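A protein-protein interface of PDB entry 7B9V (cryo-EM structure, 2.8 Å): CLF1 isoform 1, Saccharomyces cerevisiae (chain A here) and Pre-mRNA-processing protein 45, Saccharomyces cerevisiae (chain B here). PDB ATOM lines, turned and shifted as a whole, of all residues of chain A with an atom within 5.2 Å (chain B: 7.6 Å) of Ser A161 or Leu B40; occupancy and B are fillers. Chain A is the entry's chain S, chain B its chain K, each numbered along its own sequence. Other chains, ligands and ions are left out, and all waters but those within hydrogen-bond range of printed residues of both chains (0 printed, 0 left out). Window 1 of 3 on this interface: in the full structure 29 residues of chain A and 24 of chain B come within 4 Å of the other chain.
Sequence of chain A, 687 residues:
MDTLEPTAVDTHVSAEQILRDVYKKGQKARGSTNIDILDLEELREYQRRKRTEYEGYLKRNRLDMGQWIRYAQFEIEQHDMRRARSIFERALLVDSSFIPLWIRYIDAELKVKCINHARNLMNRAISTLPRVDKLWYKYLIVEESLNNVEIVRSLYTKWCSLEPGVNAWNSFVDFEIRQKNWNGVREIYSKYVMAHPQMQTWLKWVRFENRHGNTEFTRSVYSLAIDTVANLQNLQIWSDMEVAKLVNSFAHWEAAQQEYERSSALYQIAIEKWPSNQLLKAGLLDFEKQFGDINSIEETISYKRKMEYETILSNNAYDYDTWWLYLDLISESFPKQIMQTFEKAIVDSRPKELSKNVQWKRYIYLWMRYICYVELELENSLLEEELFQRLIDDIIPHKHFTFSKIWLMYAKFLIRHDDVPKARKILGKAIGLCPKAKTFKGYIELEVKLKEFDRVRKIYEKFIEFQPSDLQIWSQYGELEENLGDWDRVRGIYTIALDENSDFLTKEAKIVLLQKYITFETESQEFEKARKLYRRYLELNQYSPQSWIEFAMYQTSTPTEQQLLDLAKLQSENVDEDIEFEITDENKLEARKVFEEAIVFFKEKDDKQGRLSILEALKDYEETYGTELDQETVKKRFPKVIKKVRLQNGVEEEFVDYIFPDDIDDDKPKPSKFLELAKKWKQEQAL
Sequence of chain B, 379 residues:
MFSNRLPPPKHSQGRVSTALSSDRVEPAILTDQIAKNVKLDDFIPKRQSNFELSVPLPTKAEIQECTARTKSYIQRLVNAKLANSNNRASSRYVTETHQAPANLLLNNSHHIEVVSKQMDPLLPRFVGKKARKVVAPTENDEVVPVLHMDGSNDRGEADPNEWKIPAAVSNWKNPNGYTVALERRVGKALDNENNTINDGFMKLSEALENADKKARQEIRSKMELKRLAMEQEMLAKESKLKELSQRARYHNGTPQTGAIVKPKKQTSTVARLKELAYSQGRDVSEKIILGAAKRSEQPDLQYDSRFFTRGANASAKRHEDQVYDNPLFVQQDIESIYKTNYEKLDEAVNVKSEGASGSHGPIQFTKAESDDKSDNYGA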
ATOM      1  N   TYR A 156      -0.407  -2.295  -2.864  1.00  0.00           N
ATOM      2  CA  TYR A 156       0.731  -2.879  -2.162  1.00  0.00           C
ATOM      3  C   TYR A 156       0.410  -3.120  -0.693  1.00  0.00           C
ATOM      4  O   TYR A 156       0.900  -4.086  -0.097  1.00  0.00           O
ATOM      5  CB  TYR A 156       1.957  -1.992  -2.296  1.00  0.00           C
ATOM      6  CG  TYR A 156       2.845  -2.262  -3.486  1.00  0.00           C
ATOM      7  CD1 TYR A 156       3.489  -3.490  -3.618  1.00  0.00           C
ATOM      8  CD2 TYR A 156       3.084  -1.283  -4.441  1.00  0.00           C
ATOM      9  CE1 TYR A 156       4.320  -3.744  -4.686  1.00  0.00           C
ATOM     10  CE2 TYR A 156       3.917  -1.529  -5.514  1.00  0.00           C
ATOM     11  CZ  TYR A 156       4.526  -2.761  -5.628  1.00  0.00           C
ATOM     12  OH  TYR A 156       5.353  -3.000  -6.695  1.00  0.00           O
ATOM     13  N   THR A 157      -0.361  -2.207  -0.083  1.00  0.00           N
ATOM     14  CA  THR A 157      -0.738  -2.347   1.319  1.00  0.00           C
ATOM     15  C   THR A 157      -1.626  -3.568   1.524  1.00  0.00           C
ATOM     16  O   THR A 157      -1.439  -4.327   2.483  1.00  0.00           O
ATOM     17  CB  THR A 157      -1.445  -1.080   1.806  1.00  0.00           C
ATOM     18  OG1 THR A 157      -0.688   0.075   1.422  1.00  0.00           O
ATOM     19  CG2 THR A 157      -1.602  -1.096   3.321  1.00  0.00           C
ATOM     20  N   LYS A 158      -2.627  -3.746   0.647  1.00  0.00           N
ATOM     21  CA  LYS A 158      -3.520  -4.897   0.759  1.00  0.00           C
ATOM     22  C   LYS A 158      -2.784  -6.197   0.471  1.00  0.00           C
ATOM     23  O   LYS A 158      -3.064  -7.221   1.113  1.00  0.00           O
ATOM     24  CB  LYS A 158      -4.719  -4.729  -0.182  1.00  0.00           C
ATOM     25  CG  LYS A 158      -5.729  -5.888  -0.161  1.00  0.00           C
ATOM     26  CD  LYS A 158      -6.314  -6.146   1.215  1.00  0.00           C
ATOM     27  CE  LYS A 158      -7.325  -7.285   1.175  1.00  0.00           C
ATOM     28  NZ  LYS A 158      -8.050  -7.452   2.465  1.00  0.00           N
ATOM     29  N   TRP A 159      -1.888  -6.184  -0.530  1.00  0.00           N
ATOM     30  CA  TRP A 159      -1.126  -7.380  -0.878  1.00  0.00           C
ATOM     31  C   TRP A 159      -0.255  -7.828   0.290  1.00  0.00           C
ATOM     32  O   TRP A 159      -0.241  -9.013   0.644  1.00  0.00           O
ATOM     33  CB  TRP A 159      -0.272  -7.115  -2.120  1.00  0.00           C
ATOM     34  CG  TRP A 159       0.386  -8.340  -2.738  1.00  0.00           C
ATOM     35  CD1 TRP A 159       0.179  -9.654  -2.412  1.00  0.00           C
ATOM     36  CD2 TRP A 159       1.364  -8.344  -3.783  1.00  0.00           C
ATOM     37  NE1 TRP A 159       0.962 -10.465  -3.189  1.00  0.00           N
ATOM     38  CE2 TRP A 159       1.697  -9.688  -4.042  1.00  0.00           C
ATOM     39  CE3 TRP A 159       1.988  -7.340  -4.530  1.00  0.00           C
ATOM     40  CZ2 TRP A 159       2.624 -10.054  -5.013  1.00  0.00           C
ATOM     41  CZ3 TRP A 159       2.909  -7.704  -5.492  1.00  0.00           C
ATOM     42  CH2 TRP A 159       3.220  -9.049  -5.723  1.00  0.00           C
ATOM     43  N   CYS A 160       0.508  -6.887   0.871  1.00  0.00           N
ATOM     44  CA  CYS A 160       1.469  -7.254   1.906  1.00  0.00           C
ATOM     45  C   CYS A 160       0.796  -7.712   3.193  1.00  0.00           C
ATOM     46  O   CYS A 160       1.404  -8.455   3.969  1.00  0.00           O
ATOM     47  CB  CYS A 160       2.424  -6.096   2.177  1.00  0.00           C
ATOM     48  SG  CYS A 160       3.551  -5.766   0.806  1.00  0.00           S
ATOM     49  N   SER A 161      -0.436  -7.249   3.455  1.00  0.00           N
ATOM     50  CA  SER A 161      -1.171  -7.667   4.644  1.00  0.00           C
ATOM     51  C   SER A 161      -1.545  -9.145   4.635  1.00  0.00           C
ATOM     52  O   SER A 161      -1.768  -9.725   5.704  1.00  0.00           O
ATOM     53  CB  SER A 161      -2.438  -6.823   4.789  1.00  0.00           C
ATOM     54  OG  SER A 161      -3.404  -7.166   3.808  1.00  0.00           O
ATOM     55  N   LEU A 162      -1.599  -9.766   3.457  1.00  0.00           N
ATOM     56  CA  LEU A 162      -1.953 -11.171   3.282  1.00  0.00           C
ATOM     57  C   LEU A 162      -0.775 -12.123   3.400  1.00  0.00           C
ATOM     58  O   LEU A 162      -0.928 -13.285   3.006  1.00  0.00           O
ATOM     59  CB  LEU A 162      -2.631 -11.382   1.928  1.00  0.00           C
ATOM     60  CG  LEU A 162      -3.934 -10.623   1.700  1.00  0.00           C
ATOM     61  CD1 LEU A 162      -4.335 -10.690   0.238  1.00  0.00           C
ATOM     62  CD2 LEU A 162      -5.019 -11.176   2.605  1.00  0.00           C
ATOM     63  N   GLU A 163       0.374 -11.660   3.911  1.00  0.00           N
ATOM     64  CA  GLU A 163       1.612 -12.428   4.108  1.00  0.00           C
ATOM     65  C   GLU A 163       2.095 -13.069   2.796  1.00  0.00           C
ATOM     66  O   GLU A 163       2.134 -14.303   2.704  1.00  0.00           O
ATOM     67  CB  GLU A 163       1.447 -13.479   5.203  1.00  0.00           C
ATOM     68  CG  GLU A 163       1.188 -12.861   6.556  1.00  0.00           C
ATOM     69  CD  GLU A 163       1.551 -13.803   7.665  1.00  0.00           C
ATOM     70  OE1 GLU A 163       1.131 -14.975   7.582  1.00  0.00           O
ATOM     71  OE2 GLU A 163       2.265 -13.387   8.603  1.00  0.00           O
ATOM     72  N   PRO A 164       2.462 -12.299   1.759  1.00  0.00           N
ATOM     73  CA  PRO A 164       3.056 -12.895   0.558  1.00  0.00           C
ATOM     74  C   PRO A 164       4.522 -13.247   0.770  1.00  0.00           C
ATOM     75  O   PRO A 164       5.081 -13.074   1.846  1.00  0.00           O
ATOM     76  CB  PRO A 164       2.926 -11.789  -0.485  1.00  0.00           C
ATOM     77  CG  PRO A 164       3.025 -10.610   0.311  1.00  0.00           C
ATOM     78  CD  PRO A 164       2.377 -10.840   1.568  1.00  0.00           C
ATOM     79  N   ASN B  37     -12.921  -9.664  -0.373  1.00  0.00           N
ATOM     80  CA  ASN B  37     -13.291 -11.021   0.002  1.00  0.00           C
ATOM     81  C   ASN B  37     -12.128 -11.770   0.651  1.00  0.00           C
ATOM     82  O   ASN B  37     -12.356 -12.793   1.303  1.00  0.00           O
ATOM     83  CB  ASN B  37     -13.793 -11.780  -1.223  1.00  0.00           C
ATOM     84  CG  ASN B  37     -14.827 -11.001  -1.996  1.00  0.00           C
ATOM     85  OD1 ASN B  37     -14.493 -10.203  -2.868  1.00  0.00           O
ATOM     86  ND2 ASN B  37     -16.097 -11.239  -1.691  1.00  0.00           N
ATOM     87  N   VAL B  38     -10.896 -11.281   0.494  1.00  0.00           N
ATOM     88  CA  VAL B  38      -9.697 -11.973   0.953  1.00  0.00           C
ATOM     89  C   VAL B  38      -9.252 -11.344   2.267  1.00  0.00           C
ATOM     90  O   VAL B  38      -9.126 -10.117   2.369  1.00  0.00           O
ATOM     91  CB  VAL B  38      -8.575 -11.915  -0.098  1.00  0.00           C
ATOM     92  CG1 VAL B  38      -7.460 -12.904   0.254  1.00  0.00           C
ATOM     93  CG2 VAL B  38      -9.126 -12.203  -1.483  1.00  0.00           C
ATOM     94  N   LYS B  39      -8.989 -12.182   3.264  1.00  0.00           N
ATOM     95  CA  LYS B  39      -8.551 -11.727   4.577  1.00  0.00           C
ATOM     96  C   LYS B  39      -7.599 -12.761   5.163  1.00  0.00           C
ATOM     97  O   LYS B  39      -7.729 -13.955   4.882  1.00  0.00           O
ATOM     98  CB  LYS B  39      -9.766 -11.451   5.475  1.00  0.00           C
ATOM     99  CG  LYS B  39     -10.594 -12.673   5.848  1.00  0.00           C
ATOM    100  CD  LYS B  39     -12.061 -12.305   6.051  1.00  0.00           C
ATOM    101  CE  LYS B  39     -12.751 -12.091   4.708  1.00  0.00           C
ATOM    102  NZ  LYS B  39     -13.206 -13.370   4.086  1.00  0.00           N
ATOM    103  N   LEU B  40      -6.584 -12.284   5.900  1.00  0.00           N
ATOM    104  CA  LEU B  40      -5.608 -13.187   6.512  1.00  0.00           C
ATOM    105  C   LEU B  40      -6.230 -14.111   7.561  1.00  0.00           C
ATOM    106  O   LEU B  40      -5.710 -15.215   7.784  1.00  0.00           O
ATOM    107  CB  LEU B  40      -4.461 -12.369   7.120  1.00  0.00           C
ATOM    108  CG  LEU B  40      -3.279 -13.071   7.809  1.00  0.00           C
ATOM    109  CD1 LEU B  40      -2.536 -13.972   6.828  1.00  0.00           C
ATOM    110  CD2 LEU B  40      -2.326 -12.090   8.473  1.00  0.00           C
ATOM    111  N   ASP B  41      -7.331 -13.682   8.216  1.00  0.00           N
ATOM    112  CA  ASP B  41      -8.013 -14.495   9.232  1.00  0.00           C
ATOM    113  C   ASP B  41      -8.504 -15.839   8.671  1.00  0.00           C
ATOM    114  O   ASP B  41      -8.565 -16.827   9.408  1.00  0.00           O
ATOM    115  CB  ASP B  41      -9.186 -13.676   9.813  1.00  0.00           C
ATOM    116  CG  ASP B  41      -9.925 -14.382  10.958  1.00  0.00           C
ATOM    117  OD1 ASP B  41      -9.341 -15.250  11.635  1.00  0.00           O
ATOM    118  OD2 ASP B  41     -11.127 -14.084  11.151  1.00  0.00           O
ATOM    119  N   ASP B  42      -8.741 -15.923   7.354  1.00  0.00           N
ATOM    120  CA  ASP B  42      -9.160 -17.165   6.716  1.00  0.00           C
ATOM    121  C   ASP B  42      -8.002 -18.123   6.433  1.00  0.00           C
ATOM    122  O   ASP B  42      -8.208 -19.338   6.452  1.00  0.00           O
ATOM    123  CB  ASP B  42      -9.910 -16.870   5.414  1.00  0.00           C
ATOM    124  CG  ASP B  42     -11.291 -16.281   5.648  1.00  0.00           C
ATOM    125  OD1 ASP B  42     -11.819 -16.433   6.769  1.00  0.00           O
ATOM    126  OD2 ASP B  42     -11.858 -15.686   4.706  1.00  0.00           O
ATOM    127  N   PHE B  43      -6.784 -17.608   6.189  1.00  0.00           N
ATOM    128  CA  PHE B  43      -5.618 -18.473   5.964  1.00  0.00           C
ATOM    129  C   PHE B  43      -5.076 -19.123   7.238  1.00  0.00           C
ATOM    130  O   PHE B  43      -4.555 -20.244   7.184  1.00  0.00           O
ATOM    131  CB  PHE B  43      -4.458 -17.656   5.366  1.00  0.00           C
ATOM    132  CG  PHE B  43      -4.634 -17.201   3.922  1.00  0.00           C
ATOM    133  CD1 PHE B  43      -4.164 -17.982   2.870  1.00  0.00           C
ATOM    134  CD2 PHE B  43      -5.186 -15.957   3.631  1.00  0.00           C
ATOM    135  CE1 PHE B  43      -4.277 -17.544   1.548  1.00  0.00           C
ATOM    136  CE2 PHE B  43      -5.302 -15.517   2.311  1.00  0.00           C
ATOM    137  CZ  PHE B  43      -4.840 -16.312   1.276  1.00  0.00           C
ATOM    138  N   ILE B  44      -5.161 -18.436   8.372  1.00  0.00           N
ATOM    139  CA  ILE B  44      -4.567 -18.892   9.635  1.00  0.00           C
ATOM    140  C   ILE B  44      -5.401 -20.018  10.246  1.00  0.00           C
ATOM    141  O   ILE B  44      -6.619 -19.849  10.425  1.00  0.00           O
ATOM    142  CB  ILE B  44      -4.427 -17.719  10.599  1.00  0.00           C
ATOM    143  CG1 ILE B  44      -3.354 -16.757  10.083  1.00  0.00           C
ATOM    144  CG2 ILE B  44      -4.078 -18.189  12.004  1.00  0.00           C
ATOM    145  CD1 ILE B  44      -3.308 -15.440  10.815  1.00  0.00           C
ATOM    146  N   PRO B  45      -4.795 -21.167  10.567  1.00  0.00           N
ATOM    147  CA  PRO B  45      -5.512 -22.222  11.303  1.00  0.00           C
ATOM    148  C   PRO B  45      -5.834 -21.798  12.738  1.00  0.00           C
ATOM    149  O   PRO B  45      -4.987 -21.245  13.442  1.00  0.00           O
ATOM    150  CB  PRO B  45      -4.539 -23.403  11.260  1.00  0.00           C
ATOM    151  CG  PRO B  45      -3.207 -22.799  11.095  1.00  0.00           C
ATOM    152  CD  PRO B  45      -3.412 -21.563  10.267  1.00  0.00           C
ATOM    153  N   LYS B  46      -7.077 -22.056  13.165  1.00  0.00           N
ATOM    154  CA  LYS B  46      -7.546 -21.574  14.468  1.00  0.00           C
ATOM    155  C   LYS B  46      -6.967 -22.345  15.656  1.00  0.00           C
ATOM    156  O   LYS B  46      -6.776 -21.763  16.729  1.00  0.00           O
ATOM    157  CB  LYS B  46      -9.075 -21.628  14.500  1.00  0.00           C
ATOM    158  CG  LYS B  46      -9.750 -20.472  13.779  1.00  0.00           C
ATOM    159  CD  LYS B  46      -9.838 -19.235  14.649  1.00  0.00           C
ATOM    160  CE  LYS B  46     -10.314 -18.036  13.844  1.00  0.00           C
ATOM    161  NZ  LYS B  46      -9.309 -17.602  12.835  1.00  0.00           N
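The backbone carbonyl oxygen (O) of Val B38 lies within hydrogen-bond range of the side-chain amino group (NZ) of Lys A158, at 2.9 Å.
Ser A161 touches Leu B40. Leu A162 touches Val B38 (CD2 to CG1, 3.8 Å). Lys B39 touches Leu A162 (C to CD2, 3.96 Å). Leu B40 touches Leu A162 (N to CD2, 3.8 Å). Glu A163 touches Leu B40.
Ser A161 touches one residue of chain B. Leu B40 touches three residues of chain A. Of the printed residues of chain A, Lys B39 touches Leu A162 (3.96 Å). Printed residues of chain B within 4 Å of Lys A158: Val B38 (2.9 Å). Lys B46 touches none of the printed residues of chain A. The nearest printed residue of chain A that does not touch Leu B40 is Lys A158 (6.1 Å). The nearest printed residue of chain A that does not touch Val B38 is Ser A161 (6.6 Å).
The backbone carbonyl oxygen (O) of Asn B37 is in hydrogen-bond range of the side-chain amino group (NZ) of Lys B39 (3.0 Å). The side-chain carboxylate (OD2) of Asp B42 is in salt-bridge range of the side-chain amino group (NZ) of Lys B39, at 2.8 Å. The backbone carbonyl oxygen of Lys A158 lies within hydrogen-bond range of the side-chain hydroxyl of Ser A161 (2.7 Å).
Of the 9 printed residues of chain A, 4 touch a printed residue of chain B. Printed residues of chain A that touch a printed residue of chain B: Lys A158, Ser A161, Leu A162 and Glu A163. Hydrophobic or aromatic side chains of chain A that line the printed part of chain B: Leu A162. Of the 10 printed residues of chain B, 3 touch a printed residue of chain A. Among the printed residues, no Asp or Glu carboxylate lies within 4 Å of a Lys or Arg side-chain nitrogen of the other chain.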
